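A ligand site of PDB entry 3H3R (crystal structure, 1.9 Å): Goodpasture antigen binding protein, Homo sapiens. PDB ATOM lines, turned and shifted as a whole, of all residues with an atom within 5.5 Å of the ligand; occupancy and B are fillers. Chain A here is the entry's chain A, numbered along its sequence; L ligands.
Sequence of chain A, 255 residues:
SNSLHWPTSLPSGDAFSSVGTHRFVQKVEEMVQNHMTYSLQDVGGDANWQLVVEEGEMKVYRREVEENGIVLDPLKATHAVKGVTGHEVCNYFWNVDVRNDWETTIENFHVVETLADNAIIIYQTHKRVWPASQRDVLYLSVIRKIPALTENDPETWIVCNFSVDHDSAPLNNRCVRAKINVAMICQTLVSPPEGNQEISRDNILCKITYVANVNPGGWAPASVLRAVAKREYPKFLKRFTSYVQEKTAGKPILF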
ATOM      1  N   PHE A  93      -3.461 -18.842 -30.876  1.00  0.00           N
ATOM      2  CA  PHE A  93      -4.353 -17.742 -30.475  1.00  0.00           C
ATOM      3  C   PHE A  93      -5.737 -18.266 -30.204  1.00  0.00           C
ATOM      4  O   PHE A  93      -6.408 -17.842 -29.260  1.00  0.00           O
ATOM      5  CB  PHE A  93      -4.433 -16.656 -31.550  1.00  0.00           C
ATOM      6  CG  PHE A  93      -5.213 -15.430 -31.115  1.00  0.00           C
ATOM      7  CD1 PHE A  93      -4.822 -14.696 -29.980  1.00  0.00           C
ATOM      8  CD2 PHE A  93      -6.345 -15.042 -31.801  1.00  0.00           C
ATOM      9  CE1 PHE A  93      -5.548 -13.553 -29.578  1.00  0.00           C
ATOM     10  CE2 PHE A  93      -7.083 -13.891 -31.403  1.00  0.00           C
ATOM     11  CZ  PHE A  93      -6.657 -13.151 -30.276  1.00  0.00           C
ATOM     12  N   ARG A  99      -4.811 -20.930 -23.326  1.00  0.00           N
ATOM     13  CA  ARG A  99      -5.147 -19.523 -23.145  1.00  0.00           C
ATOM     14  C   ARG A  99      -4.416 -18.961 -21.911  1.00  0.00           C
ATOM     15  O   ARG A  99      -3.845 -17.873 -21.937  1.00  0.00           O
ATOM     16  CB  ARG A  99      -6.679 -19.371 -23.012  1.00  0.00           C
ATOM     17  CG  ARG A  99      -7.192 -17.976 -22.654  1.00  0.00           C
ATOM     18  CD  ARG A  99      -7.246 -17.015 -23.838  1.00  0.00           C
ATOM     19  NE  ARG A  99      -7.231 -17.681 -25.125  1.00  0.00           N
ATOM     20  CZ  ARG A  99      -8.277 -17.874 -25.900  1.00  0.00           C
ATOM     21  NH1 ARG A  99      -8.129 -18.495 -27.049  1.00  0.00           N
ATOM     22  NH2 ARG A  99      -9.470 -17.429 -25.568  1.00  0.00           N
ATOM     23  N   TRP A 102      -0.704 -17.623 -21.783  1.00  0.00           N
ATOM     24  CA  TRP A 102      -0.283 -16.319 -22.274  1.00  0.00           C
ATOM     25  C   TRP A 102      -1.183 -15.133 -21.929  1.00  0.00           C
ATOM     26  O   TRP A 102      -0.709 -13.996 -21.874  1.00  0.00           O
ATOM     27  CB  TRP A 102      -0.042 -16.386 -23.801  1.00  0.00           C
ATOM     28  CG  TRP A 102      -1.268 -16.779 -24.594  1.00  0.00           C
ATOM     29  CD1 TRP A 102      -1.649 -18.044 -25.010  1.00  0.00           C
ATOM     30  CD2 TRP A 102      -2.310 -15.887 -25.037  1.00  0.00           C
ATOM     31  NE1 TRP A 102      -2.857 -17.976 -25.685  1.00  0.00           N
ATOM     32  CE2 TRP A 102      -3.272 -16.661 -25.729  1.00  0.00           C
ATOM     33  CE3 TRP A 102      -2.496 -14.498 -24.948  1.00  0.00           C
ATOM     34  CZ2 TRP A 102      -4.412 -16.093 -26.299  1.00  0.00           C
ATOM     35  CZ3 TRP A 102      -3.631 -13.948 -25.494  1.00  0.00           C
ATOM     36  CH2 TRP A 102      -4.561 -14.735 -26.175  1.00  0.00           C
ATOM     37  N   GLU A 103      -2.478 -15.370 -21.738  1.00  0.00           N
ATOM     38  CA  GLU A 103      -3.447 -14.317 -21.507  1.00  0.00           C
ATOM     39  C   GLU A 103      -3.334 -13.849 -20.042  1.00  0.00           C
ATOM     40  O   GLU A 103      -3.261 -14.661 -19.129  1.00  0.00           O
ATOM     41  CB  GLU A 103      -4.846 -14.846 -21.864  1.00  0.00           C
ATOM     42  CG  GLU A 103      -6.047 -14.011 -21.478  1.00  0.00           C
ATOM     43  CD  GLU A 103      -6.090 -12.646 -22.160  1.00  0.00           C
ATOM     44  OE1 GLU A 103      -6.770 -12.510 -23.187  1.00  0.00           O
ATOM     45  OE2 GLU A 103      -5.451 -11.713 -21.657  1.00  0.00           O
ATOM     46  N   THR A 105      -5.251 -10.852 -18.845  1.00  0.00           N
ATOM     47  CA  THR A 105      -6.249  -9.827 -18.497  1.00  0.00           C
ATOM     48  C   THR A 105      -7.585 -10.406 -18.121  1.00  0.00           C
ATOM     49  O   THR A 105      -8.555  -9.655 -17.968  1.00  0.00           O
ATOM     50  CB  THR A 105      -6.493  -8.840 -19.658  1.00  0.00           C
ATOM     51  OG1 THR A 105      -7.210  -9.498 -20.705  1.00  0.00           O
ATOM     52  CG2 THR A 105      -5.179  -8.326 -20.193  1.00  0.00           C
ATOM     53  N   ILE A 106      -7.625 -11.723 -18.007  1.00  0.00           N
ATOM     54  CA  ILE A 106      -8.846 -12.454 -17.781  1.00  0.00           C
ATOM     55  C   ILE A 106      -8.872 -12.923 -16.335  1.00  0.00           C
ATOM     56  O   ILE A 106      -7.847 -13.372 -15.788  1.00  0.00           O
ATOM     57  CB  ILE A 106      -8.901 -13.717 -18.639  1.00  0.00           C
ATOM     58  CG1 ILE A 106      -9.344 -13.419 -20.055  1.00  0.00           C
ATOM     59  CG2 ILE A 106      -9.876 -14.703 -18.061  1.00  0.00           C
ATOM     60  CD1 ILE A 106      -9.231 -14.661 -20.933  1.00  0.00           C
ATOM     61  N   GLN A 124     -16.198 -14.879 -20.852  1.00  0.00           N
ATOM     62  CA  GLN A 124     -15.083 -14.591 -19.943  1.00  0.00           C
ATOM     63  C   GLN A 124     -15.250 -13.268 -19.224  1.00  0.00           C
ATOM     64  O   GLN A 124     -15.903 -12.337 -19.730  1.00  0.00           O
ATOM     65  CB  GLN A 124     -13.729 -14.645 -20.681  1.00  0.00           C
ATOM     66  CG  GLN A 124     -13.432 -13.508 -21.630  1.00  0.00           C
ATOM     67  CD  GLN A 124     -12.296 -13.865 -22.595  1.00  0.00           C
ATOM     68  OE1 GLN A 124     -12.144 -15.005 -22.985  1.00  0.00           O
ATOM     69  NE2 GLN A 124     -11.565 -12.865 -23.032  1.00  0.00           N
ATOM     70  N   HIS A 126     -13.093 -10.116 -17.263  1.00  0.00           N
ATOM     71  CA  HIS A 126     -11.777  -9.588 -17.282  1.00  0.00           C
ATOM     72  C   HIS A 126     -11.394  -8.943 -15.936  1.00  0.00           C
ATOM     73  O   HIS A 126     -12.259  -8.508 -15.175  1.00  0.00           O
ATOM     74  CB  HIS A 126     -11.623  -8.606 -18.449  1.00  0.00           C
ATOM     75  CG  HIS A 126     -11.575  -9.279 -19.788  1.00  0.00           C
ATOM     76  ND1 HIS A 126     -10.391  -9.574 -20.434  1.00  0.00           N
ATOM     77  CD2 HIS A 126     -12.557  -9.758 -20.593  1.00  0.00           C
ATOM     78  CE1 HIS A 126     -10.654 -10.191 -21.571  1.00  0.00           C
ATOM     79  NE2 HIS A 126     -11.958 -10.299 -21.706  1.00  0.00           N
ATOM     80  N   VAL A 129      -9.012  -3.837 -15.309  1.00  0.00           N
ATOM     81  CA  VAL A 129      -7.954  -3.005 -15.845  1.00  0.00           C
ATOM     82  C   VAL A 129      -8.375  -1.558 -16.031  1.00  0.00           C
ATOM     83  O   VAL A 129      -7.550  -0.678 -16.249  1.00  0.00           O
ATOM     84  CB  VAL A 129      -7.432  -3.597 -17.181  1.00  0.00           C
ATOM     85  CG1 VAL A 129      -6.991  -5.027 -16.945  1.00  0.00           C
ATOM     86  CG2 VAL A 129      -8.529  -3.583 -18.221  1.00  0.00           C
ATOM     87  N   TRP A 130      -9.675  -1.294 -15.967  1.00  0.00           N
ATOM     88  CA  TRP A 130     -10.179   0.070 -16.089  1.00  0.00           C
ATOM     89  C   TRP A 130     -10.649   0.603 -14.712  1.00  0.00           C
ATOM     90  O   TRP A 130     -11.028  -0.187 -13.835  1.00  0.00           O
ATOM     91  CB  TRP A 130     -11.353   0.134 -17.072  1.00  0.00           C
ATOM     92  CG  TRP A 130     -10.994  -0.180 -18.513  1.00  0.00           C
ATOM     93  CD1 TRP A 130      -9.799   0.079 -19.161  1.00  0.00           C
ATOM     94  CD2 TRP A 130     -11.858  -0.771 -19.499  1.00  0.00           C
ATOM     95  NE1 TRP A 130      -9.876  -0.352 -20.483  1.00  0.00           N
ATOM     96  CE2 TRP A 130     -11.133  -0.866 -20.709  1.00  0.00           C
ATOM     97  CE3 TRP A 130     -13.186  -1.229 -19.463  1.00  0.00           C
ATOM     98  CZ2 TRP A 130     -11.688  -1.399 -21.874  1.00  0.00           C
ATOM     99  CZ3 TRP A 130     -13.734  -1.750 -20.625  1.00  0.00           C
ATOM    100  CH2 TRP A 130     -12.985  -1.839 -21.815  1.00  0.00           C
ATOM    101  N   ARG A 135     -15.840  -5.787 -16.487  1.00  0.00           N
ATOM    102  CA  ARG A 135     -16.466  -6.167 -17.754  1.00  0.00           C
ATOM    103  C   ARG A 135     -16.441  -7.668 -17.982  1.00  0.00           C
ATOM    104  O   ARG A 135     -15.496  -8.376 -17.564  1.00  0.00           O
ATOM    105  CB  ARG A 135     -15.753  -5.505 -18.909  1.00  0.00           C
ATOM    106  CG  ARG A 135     -16.379  -4.228 -19.369  1.00  0.00           C
ATOM    107  CD  ARG A 135     -16.301  -3.131 -18.310  1.00  0.00           C
ATOM    108  NE  ARG A 135     -16.856  -1.918 -18.861  1.00  0.00           N
ATOM    109  CZ  ARG A 135     -17.333  -0.901 -18.158  1.00  0.00           C
ATOM    110  NH1 ARG A 135     -17.301  -0.927 -16.826  1.00  0.00           N
ATOM    111  NH2 ARG A 135     -17.832   0.152 -18.817  1.00  0.00           N
ATOM    112  N   ASP A 136     -17.515  -8.152 -18.608  1.00  0.00           N
ATOM    113  CA  ASP A 136     -17.492  -9.475 -19.211  1.00  0.00           C
ATOM    114  C   ASP A 136     -17.754  -9.402 -20.708  1.00  0.00           C
ATOM    115  O   ASP A 136     -18.114  -8.364 -21.238  1.00  0.00           O
ATOM    116  CB  ASP A 136     -18.419 -10.497 -18.539  1.00  0.00           C
ATOM    117  CG  ASP A 136     -19.871 -10.083 -18.534  1.00  0.00           C
ATOM    118  OD1 ASP A 136     -20.241  -9.019 -19.110  1.00  0.00           O
ATOM    119  OD2 ASP A 136     -20.652 -10.858 -17.954  1.00  0.00           O
ATOM    120  N   VAL A 137     -17.529 -10.507 -21.391  1.00  0.00           N
ATOM    121  CA  VAL A 137     -17.699 -10.536 -22.843  1.00  0.00           C
ATOM    122  C   VAL A 137     -18.099 -11.965 -23.203  1.00  0.00           C
ATOM    123  O   VAL A 137     -17.766 -12.915 -22.512  1.00  0.00           O
ATOM    124  CB  VAL A 137     -16.380 -10.055 -23.569  1.00  0.00           C
ATOM    125  CG1 VAL A 137     -15.286 -11.043 -23.343  1.00  0.00           C
ATOM    126  CG2 VAL A 137     -16.625  -9.786 -25.080  1.00  0.00           C
ATOM    127  N   TYR A 139     -18.329 -14.146 -26.734  1.00  0.00           N
ATOM    128  CA  TYR A 139     -17.890 -14.054 -28.130  1.00  0.00           C
ATOM    129  C   TYR A 139     -17.766 -15.395 -28.843  1.00  0.00           C
ATOM    130  O   TYR A 139     -17.483 -16.451 -28.215  1.00  0.00           O
ATOM    131  CB  TYR A 139     -16.576 -13.270 -28.287  1.00  0.00           C
ATOM    132  CG  TYR A 139     -15.380 -13.869 -27.589  1.00  0.00           C
ATOM    133  CD1 TYR A 139     -14.441 -14.612 -28.280  1.00  0.00           C
ATOM    134  CD2 TYR A 139     -15.144 -13.629 -26.228  1.00  0.00           C
ATOM    135  CE1 TYR A 139     -13.332 -15.151 -27.647  1.00  0.00           C
ATOM    136  CE2 TYR A 139     -14.044 -14.179 -25.567  1.00  0.00           C
ATOM    137  CZ  TYR A 139     -13.131 -14.930 -26.300  1.00  0.00           C
ATOM    138  OH  TYR A 139     -12.056 -15.506 -25.671  1.00  0.00           O
ATOM    139  N   ASN A 161     -12.739 -13.012 -33.325  1.00  0.00           N
ATOM    140  CA  ASN A 161     -13.489 -13.051 -32.061  1.00  0.00           C
ATOM    141  C   ASN A 161     -14.555 -11.944 -32.115  1.00  0.00           C
ATOM    142  O   ASN A 161     -14.222 -10.754 -32.233  1.00  0.00           O
ATOM    143  CB  ASN A 161     -12.542 -12.839 -30.874  1.00  0.00           C
ATOM    144  CG  ASN A 161     -11.550 -14.000 -30.657  1.00  0.00           C
ATOM    145  OD1 ASN A 161     -10.497 -13.794 -30.019  1.00  0.00           O
ATOM    146  ND2 ASN A 161     -11.868 -15.196 -31.134  1.00  0.00           N
ATOM    147  N   ALA A 178     -19.230  -5.960 -22.202  1.00  0.00           N
ATOM    148  CA  ALA A 178     -18.500  -5.332 -23.297  1.00  0.00           C
ATOM    149  C   ALA A 178     -18.905  -6.020 -24.620  1.00  0.00           C
ATOM    150  O   ALA A 178     -19.401  -7.146 -24.597  1.00  0.00           O
ATOM    151  CB  ALA A 178     -16.945  -5.403 -23.056  1.00  0.00           C
ATOM    152  N   ILE A 180     -17.144  -6.829 -28.630  1.00  0.00           N
ATOM    153  CA  ILE A 180     -15.865  -6.791 -29.311  1.00  0.00           C
ATOM    154  C   ILE A 180     -15.998  -7.261 -30.752  1.00  0.00           C
ATOM    155  O   ILE A 180     -16.917  -7.972 -31.084  1.00  0.00           O
ATOM    156  CB  ILE A 180     -14.810  -7.663 -28.606  1.00  0.00           C
ATOM    157  CG1 ILE A 180     -15.217  -9.128 -28.593  1.00  0.00           C
ATOM    158  CG2 ILE A 180     -14.576  -7.161 -27.136  1.00  0.00           C
ATOM    159  CD1 ILE A 180     -14.043 -10.089 -28.197  1.00  0.00           C
ATOM    160  N   VAL A 182     -12.701  -8.461 -33.006  1.00  0.00           N
ATOM    161  CA  VAL A 182     -11.249  -8.610 -33.020  1.00  0.00           C
ATOM    162  C   VAL A 182     -10.888  -9.624 -34.100  1.00  0.00           C
ATOM    163  O   VAL A 182     -11.618 -10.586 -34.328  1.00  0.00           O
ATOM    164  CB  VAL A 182     -10.750  -9.155 -31.638  1.00  0.00           C
ATOM    165  CG1 VAL A 182      -9.192  -9.439 -31.537  1.00  0.00           C
ATOM    166  CG2 VAL A 182     -11.176  -8.189 -30.477  1.00  0.00           C
ATOM    167  N   TYR A 210      -3.298  -7.465 -36.242  1.00  0.00           N
ATOM    168  CA  TYR A 210      -4.242  -7.718 -35.174  1.00  0.00           C
ATOM    169  C   TYR A 210      -5.092  -6.447 -35.087  1.00  0.00           C
ATOM    170  O   TYR A 210      -4.537  -5.354 -34.991  1.00  0.00           O
ATOM    171  CB  TYR A 210      -3.495  -7.996 -33.875  1.00  0.00           C
ATOM    172  CG  TYR A 210      -4.380  -8.064 -32.643  1.00  0.00           C
ATOM    173  CD1 TYR A 210      -4.649  -6.920 -31.870  1.00  0.00           C
ATOM    174  CD2 TYR A 210      -4.904  -9.270 -32.224  1.00  0.00           C
ATOM    175  CE1 TYR A 210      -5.472  -7.002 -30.731  1.00  0.00           C
ATOM    176  CE2 TYR A 210      -5.700  -9.346 -31.075  1.00  0.00           C
ATOM    177  CZ  TYR A 210      -5.963  -8.235 -30.353  1.00  0.00           C
ATOM    178  OH  TYR A 210      -6.766  -8.397 -29.250  1.00  0.00           O
ATOM    179  N   ALA A 212      -8.517  -4.698 -33.093  1.00  0.00           N
ATOM    180  CA  ALA A 212      -9.437  -4.883 -31.983  1.00  0.00           C
ATOM    181  C   ALA A 212     -10.373  -3.685 -31.974  1.00  0.00           C
ATOM    182  O   ALA A 212      -9.919  -2.543 -31.928  1.00  0.00           O
ATOM    183  CB  ALA A 212      -8.688  -4.957 -30.693  1.00  0.00           C
ATOM    184  N   VAL A 214     -13.287  -2.509 -29.506  1.00  0.00           N
ATOM    185  CA  VAL A 214     -13.889  -2.908 -28.252  1.00  0.00           C
ATOM    186  C   VAL A 214     -14.865  -1.801 -27.808  1.00  0.00           C
ATOM    187  O   VAL A 214     -14.475  -0.630 -27.754  1.00  0.00           O
ATOM    188  CB  VAL A 214     -12.816  -3.118 -27.180  1.00  0.00           C
ATOM    189  CG1 VAL A 214     -13.429  -3.345 -25.768  1.00  0.00           C
ATOM    190  CG2 VAL A 214     -11.901  -4.304 -27.562  1.00  0.00           C
ATOM    191  N   VAL A 228      -4.449   2.624 -20.810  1.00  0.00           N
ATOM    192  CA  VAL A 228      -4.508   1.202 -20.533  1.00  0.00           C
ATOM    193  C   VAL A 228      -4.361   0.376 -21.845  1.00  0.00           C
ATOM    194  O   VAL A 228      -3.729  -0.686 -21.854  1.00  0.00           O
ATOM    195  CB  VAL A 228      -5.823   0.833 -19.825  1.00  0.00           C
ATOM    196  CG1 VAL A 228      -6.101  -0.647 -19.935  1.00  0.00           C
ATOM    197  CG2 VAL A 228      -5.825   1.258 -18.352  1.00  0.00           C
ATOM    198  N   GLU A 232      -1.526  -2.388 -22.521  1.00  0.00           N
ATOM    199  CA  GLU A 232      -1.920  -3.789 -22.492  1.00  0.00           C
ATOM    200  C   GLU A 232      -1.837  -4.527 -23.829  1.00  0.00           C
ATOM    201  O   GLU A 232      -1.617  -5.729 -23.828  1.00  0.00           O
ATOM    202  CB  GLU A 232      -3.326  -3.941 -21.926  1.00  0.00           C
ATOM    203  CG  GLU A 232      -3.371  -3.594 -20.438  1.00  0.00           C
ATOM    204  CD  GLU A 232      -2.516  -4.526 -19.607  1.00  0.00           C
ATOM    205  OE1 GLU A 232      -2.591  -5.751 -19.850  1.00  0.00           O
ATOM    206  OE2 GLU A 232      -1.799  -4.039 -18.690  1.00  0.00           O
ATOM    207  N   TYR A 233      -2.044  -3.836 -24.946  1.00  0.00           N
ATOM    208  CA  TYR A 233      -2.027  -4.523 -26.254  1.00  0.00           C
ATOM    209  C   TYR A 233      -0.592  -4.855 -26.652  1.00  0.00           C
ATOM    210  O   TYR A 233      -0.337  -5.969 -27.098  1.00  0.00           O
ATOM    211  CB  TYR A 233      -2.723  -3.689 -27.324  1.00  0.00           C
ATOM    212  CG  TYR A 233      -4.234  -3.770 -27.228  1.00  0.00           C
ATOM    213  CD1 TYR A 233      -4.913  -4.918 -27.620  1.00  0.00           C
ATOM    214  CD2 TYR A 233      -4.970  -2.695 -26.734  1.00  0.00           C
ATOM    215  CE1 TYR A 233      -6.278  -5.002 -27.531  1.00  0.00           C
ATOM    216  CE2 TYR A 233      -6.348  -2.762 -26.650  1.00  0.00           C
ATOM    217  CZ  TYR A 233      -6.988  -3.913 -27.058  1.00  0.00           C
ATOM    218  OH  TYR A 233      -8.336  -3.984 -26.963  1.00  0.00           O
ATOM    219  N   PHE A 236       0.514  -7.787 -24.419  1.00  0.00           N
ATOM    220  CA  PHE A 236      -0.105  -9.022 -24.917  1.00  0.00           C
ATOM    221  C   PHE A 236       0.671  -9.517 -26.142  1.00  0.00           C
ATOM    222  O   PHE A 236       1.109 -10.671 -26.195  1.00  0.00           O
ATOM    223  CB  PHE A 236      -1.564  -8.724 -25.248  1.00  0.00           C
ATOM    224  CG  PHE A 236      -2.102  -9.443 -26.494  1.00  0.00           C
ATOM    225  CD1 PHE A 236      -2.116 -10.830 -26.575  1.00  0.00           C
ATOM    226  CD2 PHE A 236      -2.631  -8.708 -27.542  1.00  0.00           C
ATOM    227  CE1 PHE A 236      -2.623 -11.476 -27.744  1.00  0.00           C
ATOM    228  CE2 PHE A 236      -3.145  -9.323 -28.682  1.00  0.00           C
ATOM    229  CZ  PHE A 236      -3.118 -10.703 -28.789  1.00  0.00           C
HETATM  230  O1  LIG L   1      -7.302 -10.657 -28.071  1.00  0.00           O
HETATM  231  C1  LIG L   1      -7.181 -10.991 -26.878  1.00  0.00           C
HETATM  232  N1  LIG L   1      -7.770 -12.021 -26.225  1.00  0.00           N
HETATM  233  C2  LIG L   1      -8.781 -12.992 -26.681  1.00  0.00           C
HETATM  234  C3  LIG L   1      -8.652 -14.245 -25.803  1.00  0.00           C
HETATM  235  O2  LIG L   1      -8.923 -13.858 -24.435  1.00  0.00           O
HETATM  236  C4  LIG L   1     -10.203 -12.440 -26.523  1.00  0.00           C
HETATM  237  C5  LIG L   1     -10.048 -11.144 -27.279  1.00  0.00           C
HETATM  238  C6  LIG L   1     -10.280  -9.865 -26.565  1.00  0.00           C
HETATM  239  C7  LIG L   1     -10.830  -9.793 -25.287  1.00  0.00           C
HETATM  240  C8  LIG L   1     -10.918  -8.553 -24.668  1.00  0.00           C
HETATM  241  C9  LIG L   1     -10.456  -7.413 -25.283  1.00  0.00           C
HETATM  242  C10 LIG L   1      -9.873  -7.477 -26.538  1.00  0.00           C
HETATM  243  C11 LIG L   1      -9.776  -8.715 -27.154  1.00  0.00           C
HETATM  244  O3  LIG L   1     -10.171 -11.243 -28.702  1.00  0.00           O
HETATM  245  C12 LIG L   1      -6.176 -10.279 -26.008  1.00  0.00           C
HETATM  246  C13 LIG L   1      -6.327  -8.772 -25.937  1.00  0.00           C
HETATM  247  C14 LIG L   1      -5.388  -8.291 -24.826  1.00  0.00           C
HETATM  248  C15 LIG L   1      -5.521  -6.820 -24.416  1.00  0.00           C
HETATM  249  C16 LIG L   1      -6.796  -6.562 -23.601  1.00  0.00           C
HETATM  250  C17 LIG L   1      -7.003  -5.082 -23.316  1.00  0.00           C
HETATM  251  C18 LIG L   1      -8.013  -4.997 -22.186  1.00  0.00           C
HETATM  252  C19 LIG L   1      -9.240  -4.201 -22.605  1.00  0.00           C
HETATM  253  C20 LIG L   1     -10.384  -4.343 -21.592  1.00  0.00           C
HETATM  254  C21 LIG L   1     -10.888  -5.750 -21.338  1.00  0.00           C
HETATM  255  C22 LIG L   1     -12.397  -5.767 -21.058  1.00  0.00           C
HETATM  256  C23 LIG L   1     -13.228  -5.533 -22.314  1.00  0.00           C
HETATM  257  C24 LIG L   1     -13.873  -6.833 -22.791  1.00  0.00           C
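OH of Tyr 210 is in hydrogen-bond range of O1 of the ligand (2.6 Å). O2 of the ligand sits at hydrogen-bond distance from NE2 of Gln 124, at 3.2 Å. The side-chain amide oxygen of Asn 161 sits at hydrogen-bond distance from an oxygen (O3) of the ligand, at 2.9 Å. O2 of the ligand is in hydrogen-bond range of OE1 of Glu 103 (2.8 Å).
Residues that only touch the ligand: Trp 130, Arg 99, Phe 93, Ala 178, Val 182, His 126, Ile 106, Tyr 139, Tyr 233, Phe 236, Val 214, Val 129 and Arg 135. Within 4 Å of the ligand: Phe 93, Arg 99, Glu 103, Ile 106, Gln 124, His 126, Val 129, Trp 130, Arg 135, Tyr 139, Asn 161, Ala 178, Val 182, Tyr 210, Val 214, Tyr 233 and Phe 236. Along chain A the residues within 4 Å of the ligand span positions 93 to 236.
NE2 of His 126 sits at hydrogen-bond distance from NE2 of Gln 124, 2.9 Å away. NH1 of Arg 99 lies within hydrogen-bond range of O of Phe 93 (2.9 Å). The backbone carbonyl oxygen (O) of Asp 136 lies within hydrogen-bond range of the backbone NH (N) of Ala 178, 2.8 Å away. OH of Tyr 139 is in hydrogen-bond range of NH2 of Arg 99, 3.2 Å away. The side-chain hydroxyl (OH) of Tyr 139 lies within hydrogen-bond range of the side-chain amide oxygen (OE1) of Gln 124. OE2 of Glu 103 lies within hydrogen-bond range of N of Thr 105 (2.9 Å). The backbone NH (N) of Val 137 sits at hydrogen-bond distance from the backbone carbonyl oxygen (O) of Gln 124. A ring nitrogen (ND1) of His 126 is in hydrogen-bond range of the backbone carbonyl oxygen of Thr 105, at 3.1 Å.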
